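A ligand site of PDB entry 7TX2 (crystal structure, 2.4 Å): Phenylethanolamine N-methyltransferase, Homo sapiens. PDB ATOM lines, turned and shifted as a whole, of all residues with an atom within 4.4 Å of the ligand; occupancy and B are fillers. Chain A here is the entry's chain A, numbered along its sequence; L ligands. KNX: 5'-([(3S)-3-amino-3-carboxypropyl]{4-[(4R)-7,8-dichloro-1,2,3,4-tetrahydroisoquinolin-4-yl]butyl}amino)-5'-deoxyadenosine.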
ATOM      1  N   TYR A  39      16.639  23.342  29.011  1.00  0.00           N
ATOM      2  CA  TYR A  39      17.041  23.974  27.768  1.00  0.00           C
ATOM      3  C   TYR A  39      18.549  23.929  27.546  1.00  0.00           C
ATOM      4  O   TYR A  39      19.015  24.426  26.519  1.00  0.00           O
ATOM      5  CB  TYR A  39      16.531  25.421  27.734  1.00  0.00           C
ATOM      6  CG  TYR A  39      15.117  25.509  27.178  1.00  0.00           C
ATOM      7  CD1 TYR A  39      14.863  25.471  25.804  1.00  0.00           C
ATOM      8  CD2 TYR A  39      14.023  25.574  28.042  1.00  0.00           C
ATOM      9  CE1 TYR A  39      13.560  25.535  25.315  1.00  0.00           C
ATOM     10  CE2 TYR A  39      12.734  25.639  27.564  1.00  0.00           C
ATOM     11  CZ  TYR A  39      12.506  25.617  26.201  1.00  0.00           C
ATOM     12  OH  TYR A  39      11.209  25.662  25.763  1.00  0.00           O
ATOM     13  N   TYR A  47      15.878  20.414  16.620  1.00  0.00           N
ATOM     14  CA  TYR A  47      14.624  21.171  16.641  1.00  0.00           C
ATOM     15  C   TYR A  47      14.173  21.535  15.219  1.00  0.00           C
ATOM     16  O   TYR A  47      13.035  21.240  14.826  1.00  0.00           O
ATOM     17  CB  TYR A  47      14.798  22.419  17.497  1.00  0.00           C
ATOM     18  CG  TYR A  47      13.577  23.311  17.487  1.00  0.00           C
ATOM     19  CD1 TYR A  47      12.465  22.984  18.258  1.00  0.00           C
ATOM     20  CD2 TYR A  47      13.533  24.467  16.701  1.00  0.00           C
ATOM     21  CE1 TYR A  47      11.325  23.787  18.234  1.00  0.00           C
ATOM     22  CE2 TYR A  47      12.406  25.284  16.688  1.00  0.00           C
ATOM     23  CZ  TYR A  47      11.310  24.930  17.449  1.00  0.00           C
ATOM     24  OH  TYR A  47      10.199  25.719  17.437  1.00  0.00           O
ATOM     25  N   ASN A  51      10.417  20.224  13.228  1.00  0.00           N
ATOM     26  CA  ASN A  51       9.332  21.186  13.004  1.00  0.00           C
ATOM     27  C   ASN A  51       9.391  21.961  11.700  1.00  0.00           C
ATOM     28  O   ASN A  51       8.383  22.555  11.326  1.00  0.00           O
ATOM     29  CB  ASN A  51       9.301  22.221  14.134  1.00  0.00           C
ATOM     30  CG  ASN A  51       9.045  21.575  15.455  1.00  0.00           C
ATOM     31  OD1 ASN A  51       7.953  21.068  15.689  1.00  0.00           O
ATOM     32  ND2 ASN A  51      10.073  21.523  16.300  1.00  0.00           N
ATOM     33  N   TYR A  52      10.538  21.978  11.007  1.00  0.00           N
ATOM     34  CA  TYR A  52      10.691  22.786   9.808  1.00  0.00           C
ATOM     35  C   TYR A  52      11.309  21.998   8.653  1.00  0.00           C
ATOM     36  O   TYR A  52      11.804  22.603   7.695  1.00  0.00           O
ATOM     37  CB  TYR A  52      11.500  24.032  10.156  1.00  0.00           C
ATOM     38  CG  TYR A  52      10.780  24.850  11.204  1.00  0.00           C
ATOM     39  CD1 TYR A  52       9.672  25.618  10.852  1.00  0.00           C
ATOM     40  CD2 TYR A  52      11.153  24.806  12.546  1.00  0.00           C
ATOM     41  CE1 TYR A  52       8.983  26.343  11.784  1.00  0.00           C
ATOM     42  CE2 TYR A  52      10.448  25.545  13.497  1.00  0.00           C
ATOM     43  CZ  TYR A  52       9.363  26.306  13.106  1.00  0.00           C
ATOM     44  OH  TYR A  52       8.626  27.064  13.985  1.00  0.00           O
ATOM     45  N   ARG A  56       5.961  18.586   8.654  1.00  0.00           N
ATOM     46  CA  ARG A  56       5.551  19.911   9.098  1.00  0.00           C
ATOM     47  C   ARG A  56       6.190  21.034   8.278  1.00  0.00           C
ATOM     48  O   ARG A  56       5.593  22.114   8.126  1.00  0.00           O
ATOM     49  CB  ARG A  56       5.895  20.096  10.574  1.00  0.00           C
ATOM     50  CG  ARG A  56       5.343  19.027  11.458  1.00  0.00           C
ATOM     51  CD  ARG A  56       5.141  19.545  12.830  1.00  0.00           C
ATOM     52  NE  ARG A  56       4.354  18.614  13.629  1.00  0.00           N
ATOM     53  CZ  ARG A  56       4.328  18.628  14.969  1.00  0.00           C
ATOM     54  NH1 ARG A  56       5.056  19.516  15.640  1.00  0.00           N
ATOM     55  NH2 ARG A  56       3.583  17.745  15.629  1.00  0.00           N
ATOM     56  N   VAL A  65       0.533  23.105   8.708  1.00  0.00           N
ATOM     57  CA  VAL A  65       0.800  24.085   9.744  1.00  0.00           C
ATOM     58  C   VAL A  65       1.673  25.214   9.206  1.00  0.00           C
ATOM     59  O   VAL A  65       1.464  26.383   9.563  1.00  0.00           O
ATOM     60  CB  VAL A  65       1.442  23.411  10.972  1.00  0.00           C
ATOM     61  CG1 VAL A  65       2.800  22.744  10.654  1.00  0.00           C
ATOM     62  CG2 VAL A  65       1.553  24.423  12.120  1.00  0.00           C
ATOM     63  N   LYS A  69       0.546  29.291   9.410  1.00  0.00           N
ATOM     64  CA  LYS A  69       1.235  30.309  10.197  1.00  0.00           C
ATOM     65  C   LYS A  69       1.576  31.519   9.339  1.00  0.00           C
ATOM     66  O   LYS A  69       1.227  32.654   9.690  1.00  0.00           O
ATOM     67  CB  LYS A  69       2.499  29.729  10.824  1.00  0.00           C
ATOM     68  CG  LYS A  69       2.241  28.803  11.960  1.00  0.00           C
ATOM     69  CD  LYS A  69       3.517  28.509  12.702  1.00  0.00           C
ATOM     70  CE  LYS A  69       4.328  27.432  12.004  1.00  0.00           C
ATOM     71  NZ  LYS A  69       5.617  27.223  12.715  1.00  0.00           N
ATOM     72  N   GLY A  91      12.173  35.352  21.608  1.00  0.00           N
ATOM     73  CA  GLY A  91      12.359  33.907  21.596  1.00  0.00           C
ATOM     74  C   GLY A  91      12.438  33.286  20.210  1.00  0.00           C
ATOM     75  O   GLY A  91      11.822  32.254  19.937  1.00  0.00           O
ATOM     76  N   SER A  92      13.247  33.897  19.338  1.00  0.00           N
ATOM     77  CA  SER A  92      13.304  33.502  17.936  1.00  0.00           C
ATOM     78  C   SER A  92      13.726  32.047  17.746  1.00  0.00           C
ATOM     79  O   SER A  92      13.368  31.440  16.718  1.00  0.00           O
ATOM     80  CB  SER A  92      14.295  34.390  17.189  1.00  0.00           C
ATOM     81  OG  SER A  92      14.061  35.761  17.481  1.00  0.00           O
ATOM     82  N   GLY A  93      14.471  31.477  18.687  1.00  0.00           N
ATOM     83  CA  GLY A  93      15.138  30.221  18.445  1.00  0.00           C
ATOM     84  C   GLY A  93      16.052  30.334  17.248  1.00  0.00           C
ATOM     85  O   GLY A  93      16.672  31.376  16.999  1.00  0.00           O
ATOM     86  N   THR A  95      14.930  30.250  14.147  1.00  0.00           N
ATOM     87  CA  THR A  95      13.954  30.342  13.064  1.00  0.00           C
ATOM     88  C   THR A  95      13.769  31.785  12.626  1.00  0.00           C
ATOM     89  O   THR A  95      13.808  32.709  13.451  1.00  0.00           O
ATOM     90  CB  THR A  95      12.580  29.765  13.455  1.00  0.00           C
ATOM     91  OG1 THR A  95      11.855  30.733  14.230  1.00  0.00           O
ATOM     92  CG2 THR A  95      12.734  28.479  14.269  1.00  0.00           C
ATOM     93  N   TYR A  97      11.200  32.465   9.866  1.00  0.00           N
ATOM     94  CA  TYR A  97       9.946  32.561   9.099  1.00  0.00           C
ATOM     95  C   TYR A  97       8.959  33.545   9.710  1.00  0.00           C
ATOM     96  O   TYR A  97       8.057  34.022   8.993  1.00  0.00           O
ATOM     97  CB  TYR A  97       9.277  31.192   9.011  1.00  0.00           C
ATOM     98  CG  TYR A  97       8.706  30.755  10.362  1.00  0.00           C
ATOM     99  CD1 TYR A  97       9.505  30.094  11.277  1.00  0.00           C
ATOM    100  CD2 TYR A  97       7.395  31.050  10.729  1.00  0.00           C
ATOM    101  CE1 TYR A  97       9.010  29.714  12.501  1.00  0.00           C
ATOM    102  CE2 TYR A  97       6.892  30.676  11.963  1.00  0.00           C
ATOM    103  CZ  TYR A  97       7.707  30.001  12.849  1.00  0.00           C
ATOM    104  OH  TYR A  97       7.241  29.622  14.074  1.00  0.00           O
ATOM    105  N   GLN A  98       9.046  33.809  11.011  1.00  0.00           N
ATOM    106  CA  GLN A  98       8.029  34.643  11.624  1.00  0.00           C
ATOM    107  C   GLN A  98       8.273  36.118  11.357  1.00  0.00           C
ATOM    108  O   GLN A  98       7.439  36.953  11.719  1.00  0.00           O
ATOM    109  CB  GLN A  98       7.940  34.382  13.137  1.00  0.00           C
ATOM    110  CG  GLN A  98       9.160  34.781  13.953  1.00  0.00           C
ATOM    111  CD  GLN A  98      10.203  33.686  13.998  1.00  0.00           C
ATOM    112  OE1 GLN A  98      10.249  32.820  13.125  1.00  0.00           O
ATOM    113  NE2 GLN A  98      11.056  33.723  15.022  1.00  0.00           N
ATOM    114  N   ASP A 113      17.170  35.478  21.752  1.00  0.00           N
ATOM    115  CA  ASP A 113      16.949  34.138  22.298  1.00  0.00           C
ATOM    116  C   ASP A 113      17.749  33.916  23.575  1.00  0.00           C
ATOM    117  O   ASP A 113      18.824  34.496  23.770  1.00  0.00           O
ATOM    118  CB  ASP A 113      17.295  33.024  21.296  1.00  0.00           C
ATOM    119  CG  ASP A 113      16.629  31.693  21.668  1.00  0.00           C
ATOM    120  OD1 ASP A 113      15.379  31.638  21.765  1.00  0.00           O
ATOM    121  OD2 ASP A 113      17.354  30.697  21.895  1.00  0.00           O
ATOM    122  N   PHE A 114      17.213  33.039  24.436  1.00  0.00           N
ATOM    123  CA  PHE A 114      17.855  32.691  25.698  1.00  0.00           C
ATOM    124  C   PHE A 114      19.182  31.968  25.480  1.00  0.00           C
ATOM    125  O   PHE A 114      20.135  32.166  26.236  1.00  0.00           O
ATOM    126  CB  PHE A 114      16.888  31.833  26.516  1.00  0.00           C
ATOM    127  CG  PHE A 114      17.417  31.384  27.854  1.00  0.00           C
ATOM    128  CD1 PHE A 114      17.233  32.152  28.991  1.00  0.00           C
ATOM    129  CD2 PHE A 114      18.085  30.171  27.972  1.00  0.00           C
ATOM    130  CE1 PHE A 114      17.710  31.727  30.206  1.00  0.00           C
ATOM    131  CE2 PHE A 114      18.570  29.740  29.187  1.00  0.00           C
ATOM    132  CZ  PHE A 114      18.385  30.522  30.314  1.00  0.00           C
ATOM    133  N   LEU A 115      19.264  31.114  24.449  1.00  0.00           N
ATOM    134  CA  LEU A 115      20.420  30.250  24.205  1.00  0.00           C
ATOM    135  C   LEU A 115      21.366  30.834  23.160  1.00  0.00           C
ATOM    136  O   LEU A 115      20.936  31.292  22.098  1.00  0.00           O
ATOM    137  CB  LEU A 115      19.961  28.873  23.747  1.00  0.00           C
ATOM    138  CG  LEU A 115      19.060  28.018  24.639  1.00  0.00           C
ATOM    139  CD1 LEU A 115      18.740  26.697  23.927  1.00  0.00           C
ATOM    140  CD2 LEU A 115      19.732  27.766  25.970  1.00  0.00           C
ATOM    141  N   ASN A 118      21.450  28.939  19.756  1.00  0.00           N
ATOM    142  CA  ASN A 118      20.450  29.365  18.785  1.00  0.00           C
ATOM    143  C   ASN A 118      20.826  30.687  18.128  1.00  0.00           C
ATOM    144  O   ASN A 118      20.641  30.839  16.913  1.00  0.00           O
ATOM    145  CB  ASN A 118      19.080  29.473  19.464  1.00  0.00           C
ATOM    146  CG  ASN A 118      18.373  28.134  19.543  1.00  0.00           C
ATOM    147  OD1 ASN A 118      18.560  27.260  18.699  1.00  0.00           O
ATOM    148  ND2 ASN A 118      17.540  27.965  20.575  1.00  0.00           N
ATOM    149  N   ILE A 169      18.022  37.203  25.939  1.00  0.00           N
ATOM    150  CA  ILE A 169      16.752  37.603  26.527  1.00  0.00           C
ATOM    151  C   ILE A 169      16.350  36.528  27.529  1.00  0.00           C
ATOM    152  O   ILE A 169      16.752  35.364  27.412  1.00  0.00           O
ATOM    153  CB  ILE A 169      15.675  37.804  25.426  1.00  0.00           C
ATOM    154  CG1 ILE A 169      14.320  38.202  26.020  1.00  0.00           C
ATOM    155  CG2 ILE A 169      15.521  36.536  24.592  1.00  0.00           C
ATOM    156  CD1 ILE A 169      13.419  38.957  25.077  1.00  0.00           C
ATOM    157  N   ASP A 170      15.583  36.926  28.543  1.00  0.00           N
ATOM    158  CA  ASP A 170      14.979  35.998  29.502  1.00  0.00           C
ATOM    159  C   ASP A 170      13.629  36.603  29.861  1.00  0.00           C
ATOM    160  O   ASP A 170      13.579  37.628  30.550  1.00  0.00           O
ATOM    161  CB  ASP A 170      15.850  35.835  30.741  1.00  0.00           C
ATOM    162  CG  ASP A 170      15.315  34.776  31.716  1.00  0.00           C
ATOM    163  OD1 ASP A 170      14.085  34.566  31.807  1.00  0.00           O
ATOM    164  OD2 ASP A 170      16.137  34.154  32.411  1.00  0.00           O
ATOM    165  N   VAL A 171      12.549  35.983  29.387  1.00  0.00           N
ATOM    166  CA  VAL A 171      11.208  36.556  29.567  1.00  0.00           C
ATOM    167  C   VAL A 171      10.740  36.528  31.006  1.00  0.00           C
ATOM    168  O   VAL A 171       9.736  37.165  31.342  1.00  0.00           O
ATOM    169  CB  VAL A 171      10.183  35.843  28.647  1.00  0.00           C
ATOM    170  CG1 VAL A 171      10.584  36.003  27.192  1.00  0.00           C
ATOM    171  CG2 VAL A 171      10.067  34.381  29.010  1.00  0.00           C
ATOM    172  N   HIS A 172      11.457  35.821  31.878  1.00  0.00           N
ATOM    173  CA  HIS A 172      11.076  35.767  33.291  1.00  0.00           C
ATOM    174  C   HIS A 172      11.553  36.996  34.063  1.00  0.00           C
ATOM    175  O   HIS A 172      10.915  37.370  35.065  1.00  0.00           O
ATOM    176  CB  HIS A 172      11.601  34.467  33.904  1.00  0.00           C
ATOM    177  CG  HIS A 172      11.010  33.231  33.297  1.00  0.00           C
ATOM    178  ND1 HIS A 172       9.650  33.067  33.140  1.00  0.00           N
ATOM    179  CD2 HIS A 172      11.578  32.101  32.817  1.00  0.00           C
ATOM    180  CE1 HIS A 172       9.408  31.901  32.569  1.00  0.00           C
ATOM    181  NE2 HIS A 172      10.567  31.292  32.370  1.00  0.00           N
ATOM    182  N   ALA A 193       6.811  33.745  18.659  1.00  0.00           N
ATOM    183  CA  ALA A 193       6.249  32.491  18.184  1.00  0.00           C
ATOM    184  C   ALA A 193       6.776  31.361  19.064  1.00  0.00           C
ATOM    185  O   ALA A 193       7.984  31.084  19.052  1.00  0.00           O
ATOM    186  CB  ALA A 193       6.581  32.224  16.724  1.00  0.00           C
ATOM    187  N   PHE A 194       5.871  30.708  19.781  1.00  0.00           N
ATOM    188  CA  PHE A 194       6.113  29.450  20.489  1.00  0.00           C
ATOM    189  C   PHE A 194       7.032  29.613  21.685  1.00  0.00           C
ATOM    190  O   PHE A 194       7.703  28.676  22.098  1.00  0.00           O
ATOM    191  CB  PHE A 194       6.675  28.381  19.537  1.00  0.00           C
ATOM    192  CG  PHE A 194       5.701  27.950  18.494  1.00  0.00           C
ATOM    193  CD1 PHE A 194       4.599  27.176  18.843  1.00  0.00           C
ATOM    194  CD2 PHE A 194       5.861  28.345  17.173  1.00  0.00           C
ATOM    195  CE1 PHE A 194       3.685  26.784  17.872  1.00  0.00           C
ATOM    196  CE2 PHE A 194       4.959  27.968  16.212  1.00  0.00           C
ATOM    197  CZ  PHE A 194       3.865  27.187  16.552  1.00  0.00           C
ATOM    198  N   CYS A 195       7.074  30.815  22.245  1.00  0.00           N
ATOM    199  CA  CYS A 195       8.053  31.063  23.292  1.00  0.00           C
ATOM    200  C   CYS A 195       7.466  30.845  24.688  1.00  0.00           C
ATOM    201  O   CYS A 195       7.881  29.919  25.398  1.00  0.00           O
ATOM    202  CB  CYS A 195       8.596  32.473  23.192  1.00  0.00           C
ATOM    203  SG  CYS A 195       9.937  32.586  24.321  1.00  0.00           S
ATOM    204  N   ALA A 198       6.231  27.639  26.009  1.00  0.00           N
ATOM    205  CA  ALA A 198       7.302  26.656  25.973  1.00  0.00           C
ATOM    206  C   ALA A 198       8.359  26.871  27.045  1.00  0.00           C
ATOM    207  O   ALA A 198       9.218  25.999  27.216  1.00  0.00           O
ATOM    208  CB  ALA A 198       7.980  26.679  24.605  1.00  0.00           C
ATOM    209  N   VAL A 199       8.340  28.004  27.743  1.00  0.00           N
ATOM    210  CA  VAL A 199       9.377  28.336  28.721  1.00  0.00           C
ATOM    211  C   VAL A 199       8.817  28.531  30.131  1.00  0.00           C
ATOM    212  O   VAL A 199       9.581  28.803  31.066  1.00  0.00           O
ATOM    213  CB  VAL A 199      10.169  29.579  28.287  1.00  0.00           C
ATOM    214  CG1 VAL A 199      10.815  29.331  26.913  1.00  0.00           C
ATOM    215  CG2 VAL A 199       9.270  30.813  28.237  1.00  0.00           C
ATOM    216  N   GLU A 231      -0.361  21.693  24.673  1.00  0.00           N
ATOM    217  CA  GLU A 231       0.856  20.890  24.561  1.00  0.00           C
ATOM    218  C   GLU A 231       1.568  20.859  25.910  1.00  0.00           C
ATOM    219  O   GLU A 231       1.616  21.859  26.625  1.00  0.00           O
ATOM    220  CB  GLU A 231       1.806  21.431  23.478  1.00  0.00           C
ATOM    221  CG  GLU A 231       3.302  21.327  23.797  1.00  0.00           C
ATOM    222  CD  GLU A 231       4.237  21.895  22.703  1.00  0.00           C
ATOM    223  OE1 GLU A 231       4.428  21.214  21.664  1.00  0.00           O
ATOM    224  OE2 GLU A 231       4.762  23.028  22.868  1.00  0.00           O
ATOM    225  N   TYR A 234       7.792  18.746  24.249  1.00  0.00           N
ATOM    226  CA  TYR A 234       8.328  18.545  22.898  1.00  0.00           C
ATOM    227  C   TYR A 234       9.822  18.245  23.001  1.00  0.00           C
ATOM    228  O   TYR A 234      10.475  18.579  23.999  1.00  0.00           O
ATOM    229  CB  TYR A 234       8.105  19.763  21.972  1.00  0.00           C
ATOM    230  CG  TYR A 234       8.973  20.940  22.334  1.00  0.00           C
ATOM    231  CD1 TYR A 234       8.627  21.779  23.392  1.00  0.00           C
ATOM    232  CD2 TYR A 234      10.147  21.193  21.648  1.00  0.00           C
ATOM    233  CE1 TYR A 234       9.421  22.861  23.742  1.00  0.00           C
ATOM    234  CE2 TYR A 234      10.949  22.268  21.979  1.00  0.00           C
ATOM    235  CZ  TYR A 234      10.589  23.091  23.036  1.00  0.00           C
ATOM    236  OH  TYR A 234      11.379  24.165  23.337  1.00  0.00           O
ATOM    237  N   MET A 270      -4.470  20.512  14.750  1.00  0.00           N
ATOM    238  CA  MET A 270      -3.311  19.833  14.172  1.00  0.00           C
ATOM    239  C   MET A 270      -3.784  18.542  13.502  1.00  0.00           C
ATOM    240  O   MET A 270      -4.425  17.713  14.156  1.00  0.00           O
ATOM    241  CB  MET A 270      -2.266  19.566  15.252  1.00  0.00           C
ATOM    242  CG  MET A 270      -0.891  19.038  14.783  1.00  0.00           C
ATOM    243  SD  MET A 270       0.292  20.187  13.980  1.00  0.00           S
ATOM    244  CE  MET A 270      -0.339  21.801  14.387  1.00  0.00           C
ATOM    245  N   ASP A 279       6.237  15.744  19.730  1.00  0.00           N
ATOM    246  CA  ASP A 279       5.548  16.535  20.741  1.00  0.00           C
ATOM    247  C   ASP A 279       4.145  15.965  20.880  1.00  0.00           C
ATOM    248  O   ASP A 279       3.801  14.936  20.282  1.00  0.00           O
ATOM    249  CB  ASP A 279       5.519  18.034  20.400  1.00  0.00           C
ATOM    250  CG  ASP A 279       4.993  18.318  18.985  1.00  0.00           C
ATOM    251  OD1 ASP A 279       3.911  17.792  18.609  1.00  0.00           O
ATOM    252  OD2 ASP A 279       5.676  19.084  18.254  1.00  0.00           O
ATOM    253  N   VAL A 281       1.552  18.506  20.758  1.00  0.00           N
ATOM    254  CA  VAL A 281       0.758  19.666  20.384  1.00  0.00           C
ATOM    255  C   VAL A 281      -0.563  19.190  19.794  1.00  0.00           C
ATOM    256  O   VAL A 281      -0.609  18.231  19.009  1.00  0.00           O
ATOM    257  CB  VAL A 281       1.527  20.564  19.394  1.00  0.00           C
ATOM    258  CG1 VAL A 281       1.748  19.849  18.057  1.00  0.00           C
ATOM    259  CG2 VAL A 281       0.791  21.843  19.171  1.00  0.00           C
ATOM    260  N   VAL A 284      -2.513  25.018  17.127  1.00  0.00           N
ATOM    261  CA  VAL A 284      -1.664  26.209  17.148  1.00  0.00           C
ATOM    262  C   VAL A 284      -2.599  27.407  17.136  1.00  0.00           C
ATOM    263  O   VAL A 284      -3.566  27.442  16.355  1.00  0.00           O
ATOM    264  CB  VAL A 284      -0.691  26.280  15.934  1.00  0.00           C
ATOM    265  CG1 VAL A 284       0.154  27.542  15.993  1.00  0.00           C
ATOM    266  CG2 VAL A 284       0.220  25.065  15.875  1.00  0.00           C
HETATM  267  N1  KNX L   1      13.268  32.529  25.885  1.00  0.00           N
HETATM  268  N3  KNX L   1      14.105  29.619  27.768  1.00  0.00           N
HETATM  269  C4  KNX L   1      13.475  31.944  28.642  1.00  0.00           C
HETATM  270  C5  KNX L   1      14.190  29.206  26.528  1.00  0.00           C
HETATM  271  C6  KNX L   1      13.904  30.073  24.153  1.00  0.00           C
HETATM  272  C7  KNX L   1      12.612  29.220  22.421  1.00  0.00           C
HETATM  273  C8  KNX L   1      13.967  28.522  22.324  1.00  0.00           C
HETATM  274  C10 KNX L   1      11.409  28.307  22.346  1.00  0.00           C
HETATM  275  C13 KNX L   1      10.905  29.596  17.548  1.00  0.00           C
HETATM  276  C15 KNX L   1      10.687  26.634  20.719  1.00  0.00           C
HETATM  277  C17 KNX L   1       8.826  24.834  20.959  1.00  0.00           C
HETATM  278  C20 KNX L   1       6.718  23.810  17.846  1.00  0.00           C
HETATM  279  C21 KNX L   1       5.509  23.154  17.566  1.00  0.00           C
HETATM  280  C22 KNX L   1       4.862  22.290  18.631  1.00  0.00           C
HETATM  281  C24 KNX L   1       7.307  24.602  16.859  1.00  0.00           C
HETATM  282  C26 KNX L   1       5.538  24.091  15.346  1.00  0.00           C
HETATM  283  C1  KNX L   1      13.729  30.956  27.672  1.00  0.00           C
HETATM  284  C11 KNX L   1      11.554  28.841  19.940  1.00  0.00           C
HETATM  285  C12 KNX L   1      10.955  28.495  18.604  1.00  0.00           C
HETATM  286  C14 KNX L   1       9.883  29.114  16.524  1.00  0.00           C
HETATM  287  C16 KNX L   1       9.448  26.139  21.456  1.00  0.00           C
HETATM  288  C18 KNX L   1       8.043  24.970  19.674  1.00  0.00           C
HETATM  289  C19 KNX L   1       7.384  23.657  19.205  1.00  0.00           C
HETATM  290  C2  KNX L   1      13.599  31.319  26.347  1.00  0.00           C
HETATM  291  C23 KNX L   1       6.451  23.088  20.270  1.00  0.00           C
HETATM  292  C25 KNX L   1       6.727  24.740  15.615  1.00  0.00           C
HETATM  293  C27 KNX L   1       4.937  23.312  16.302  1.00  0.00           C
HETATM  294  C3  KNX L   1      13.045  33.378  26.889  1.00  0.00           C
HETATM  295  C9  KNX L   1      14.667  28.843  23.655  1.00  0.00           C
HETATM  296  N2  KNX L   1      13.126  33.182  28.209  1.00  0.00           N
HETATM  297  N4  KNX L   1      13.903  30.196  25.623  1.00  0.00           N
HETATM  298  N5  KNX L   1      10.898  28.055  20.993  1.00  0.00           N
HETATM  299  N6  KNX L   1       5.733  21.926  19.734  1.00  0.00           N
HETATM  300  N7  KNX L   1      13.557  31.734  29.962  1.00  0.00           N
HETATM  301  N8  KNX L   1      10.426  30.873  18.140  1.00  0.00           N
HETATM  302  O1  KNX L   1      12.580  29.855  23.719  1.00  0.00           O
HETATM  303  O2  KNX L   1      14.701  29.005  21.200  1.00  0.00           O
HETATM  304  O3  KNX L   1      16.048  29.065  23.512  1.00  0.00           O
HETATM  305  O4  KNX L   1      10.054  27.957  16.074  1.00  0.00           O
HETATM  306  O5  KNX L   1       8.927  29.889  16.259  1.00  0.00           O
HETATM  307 CL1  KNX L   1       3.441  22.530  15.899  1.00  0.00          CL
HETATM  308 CL2  KNX L   1       4.775  24.258  13.791  1.00  0.00          CL
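The side-chain sulfur (SG) of Cys 195 is in hydrogen-bond range of a nitrogen (N1) of the ligand (3.7 Å).
O of Gly 91 sits at hydrogen-bond distance from N8 of the ligand (2.7 Å).
The backbone carbonyl oxygen (O) of Ala 193 sits at hydrogen-bond distance from a nitrogen (N8) of the ligand (2.6 Å).
The side-chain hydroxyl (OH) of Tyr 97 sits at hydrogen-bond distance from an oxygen (O5) of the ligand (2.8 Å).
The backbone carbonyl oxygen (O) of Phe 194 sits close to a nitrogen (N5) of the ligand (3.4 Å).
OH of Tyr 47 lies within hydrogen-bond range of O4 of the ligand.
The side-chain hydroxyl of Tyr 52 is in hydrogen-bond range of an oxygen (O4) of the ligand, 2.7 Å away.
N2 of the ligand lies within hydrogen-bond range of N of Val 171.
ND2 of Asn 118 is in hydrogen-bond range of O2 of the ligand, 3.1 Å away.
OD1 of Asp 170 lies within hydrogen-bond range of N7 of the ligand (3.4 Å).
A nitrogen (N6) of the ligand is in salt-bridge range of the side-chain carboxylate of Asp 279, 3.2 Å away.
OD2 of Asp 113 lies within hydrogen-bond range of O3 of the ligand (2.6 Å).
OE1 of Glu 231 lies within salt-bridge range of N6 of the ligand (2.4 Å).
A nitrogen (N8) of the ligand sits close to the backbone carbonyl oxygen (O) of Ser 92, 3.3 Å away.
The backbone NH of His 172 is in hydrogen-bond range of the side-chain carboxylate of Asp 170.
The side-chain hydroxyl (OH) of Tyr 52 sits at hydrogen-bond distance from the side-chain amino group (NZ) of Lys 69 (3.3 Å).
OH of Tyr 39 lies within hydrogen-bond range of O of Ala 198.
The side-chain carboxylate of Asp 113 is in hydrogen-bond range of the backbone NH of Gly 93, at 3.2 Å.
ND2 of Asn 51 sits close to O of Tyr 47, at 3.3 Å.
The guanidinium group of Arg 56 is in hydrogen-bond range of the side-chain amide oxygen of Asn 51, 3.3 Å away.
OG1 of Thr 95 is in hydrogen-bond range of O of Ser 92 (3.0 Å).
The side-chain carboxylate (OD2) of Asp 279 is in salt-bridge range of the guanidinium group (NH1) of Arg 56, 2.7 Å away.
Residues that only touch the ligand: Gly 93 (3.0 Å), Tyr 234 (3.2 Å), Lys 69 (3.3 Å), Thr 95 (3.3 Å), Phe 114 (3.3 Å), Leu 115 (3.4 Å), Val 199 (3.4 Å), Arg 56 (3.4 Å), His 172 (3.5 Å), Ala 198 (3.5 Å), Val 65 (3.6 Å), Asn 51 (3.7 Å), Val 281 (3.8 Å) and Tyr 39 (3.9 Å).
Hydrophobic or aromatic side chains that line the ligand: Tyr 39, Tyr 47, Tyr 52, Val 65, Tyr 97, Phe 114, Leu 115, Val 171, His 172, Ala 193, Phe 194, Ala 198, Val 199, Tyr 234 and Val 281.
The nearest printed residue that does not touch the ligand is Val 284 (4.1 Å).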
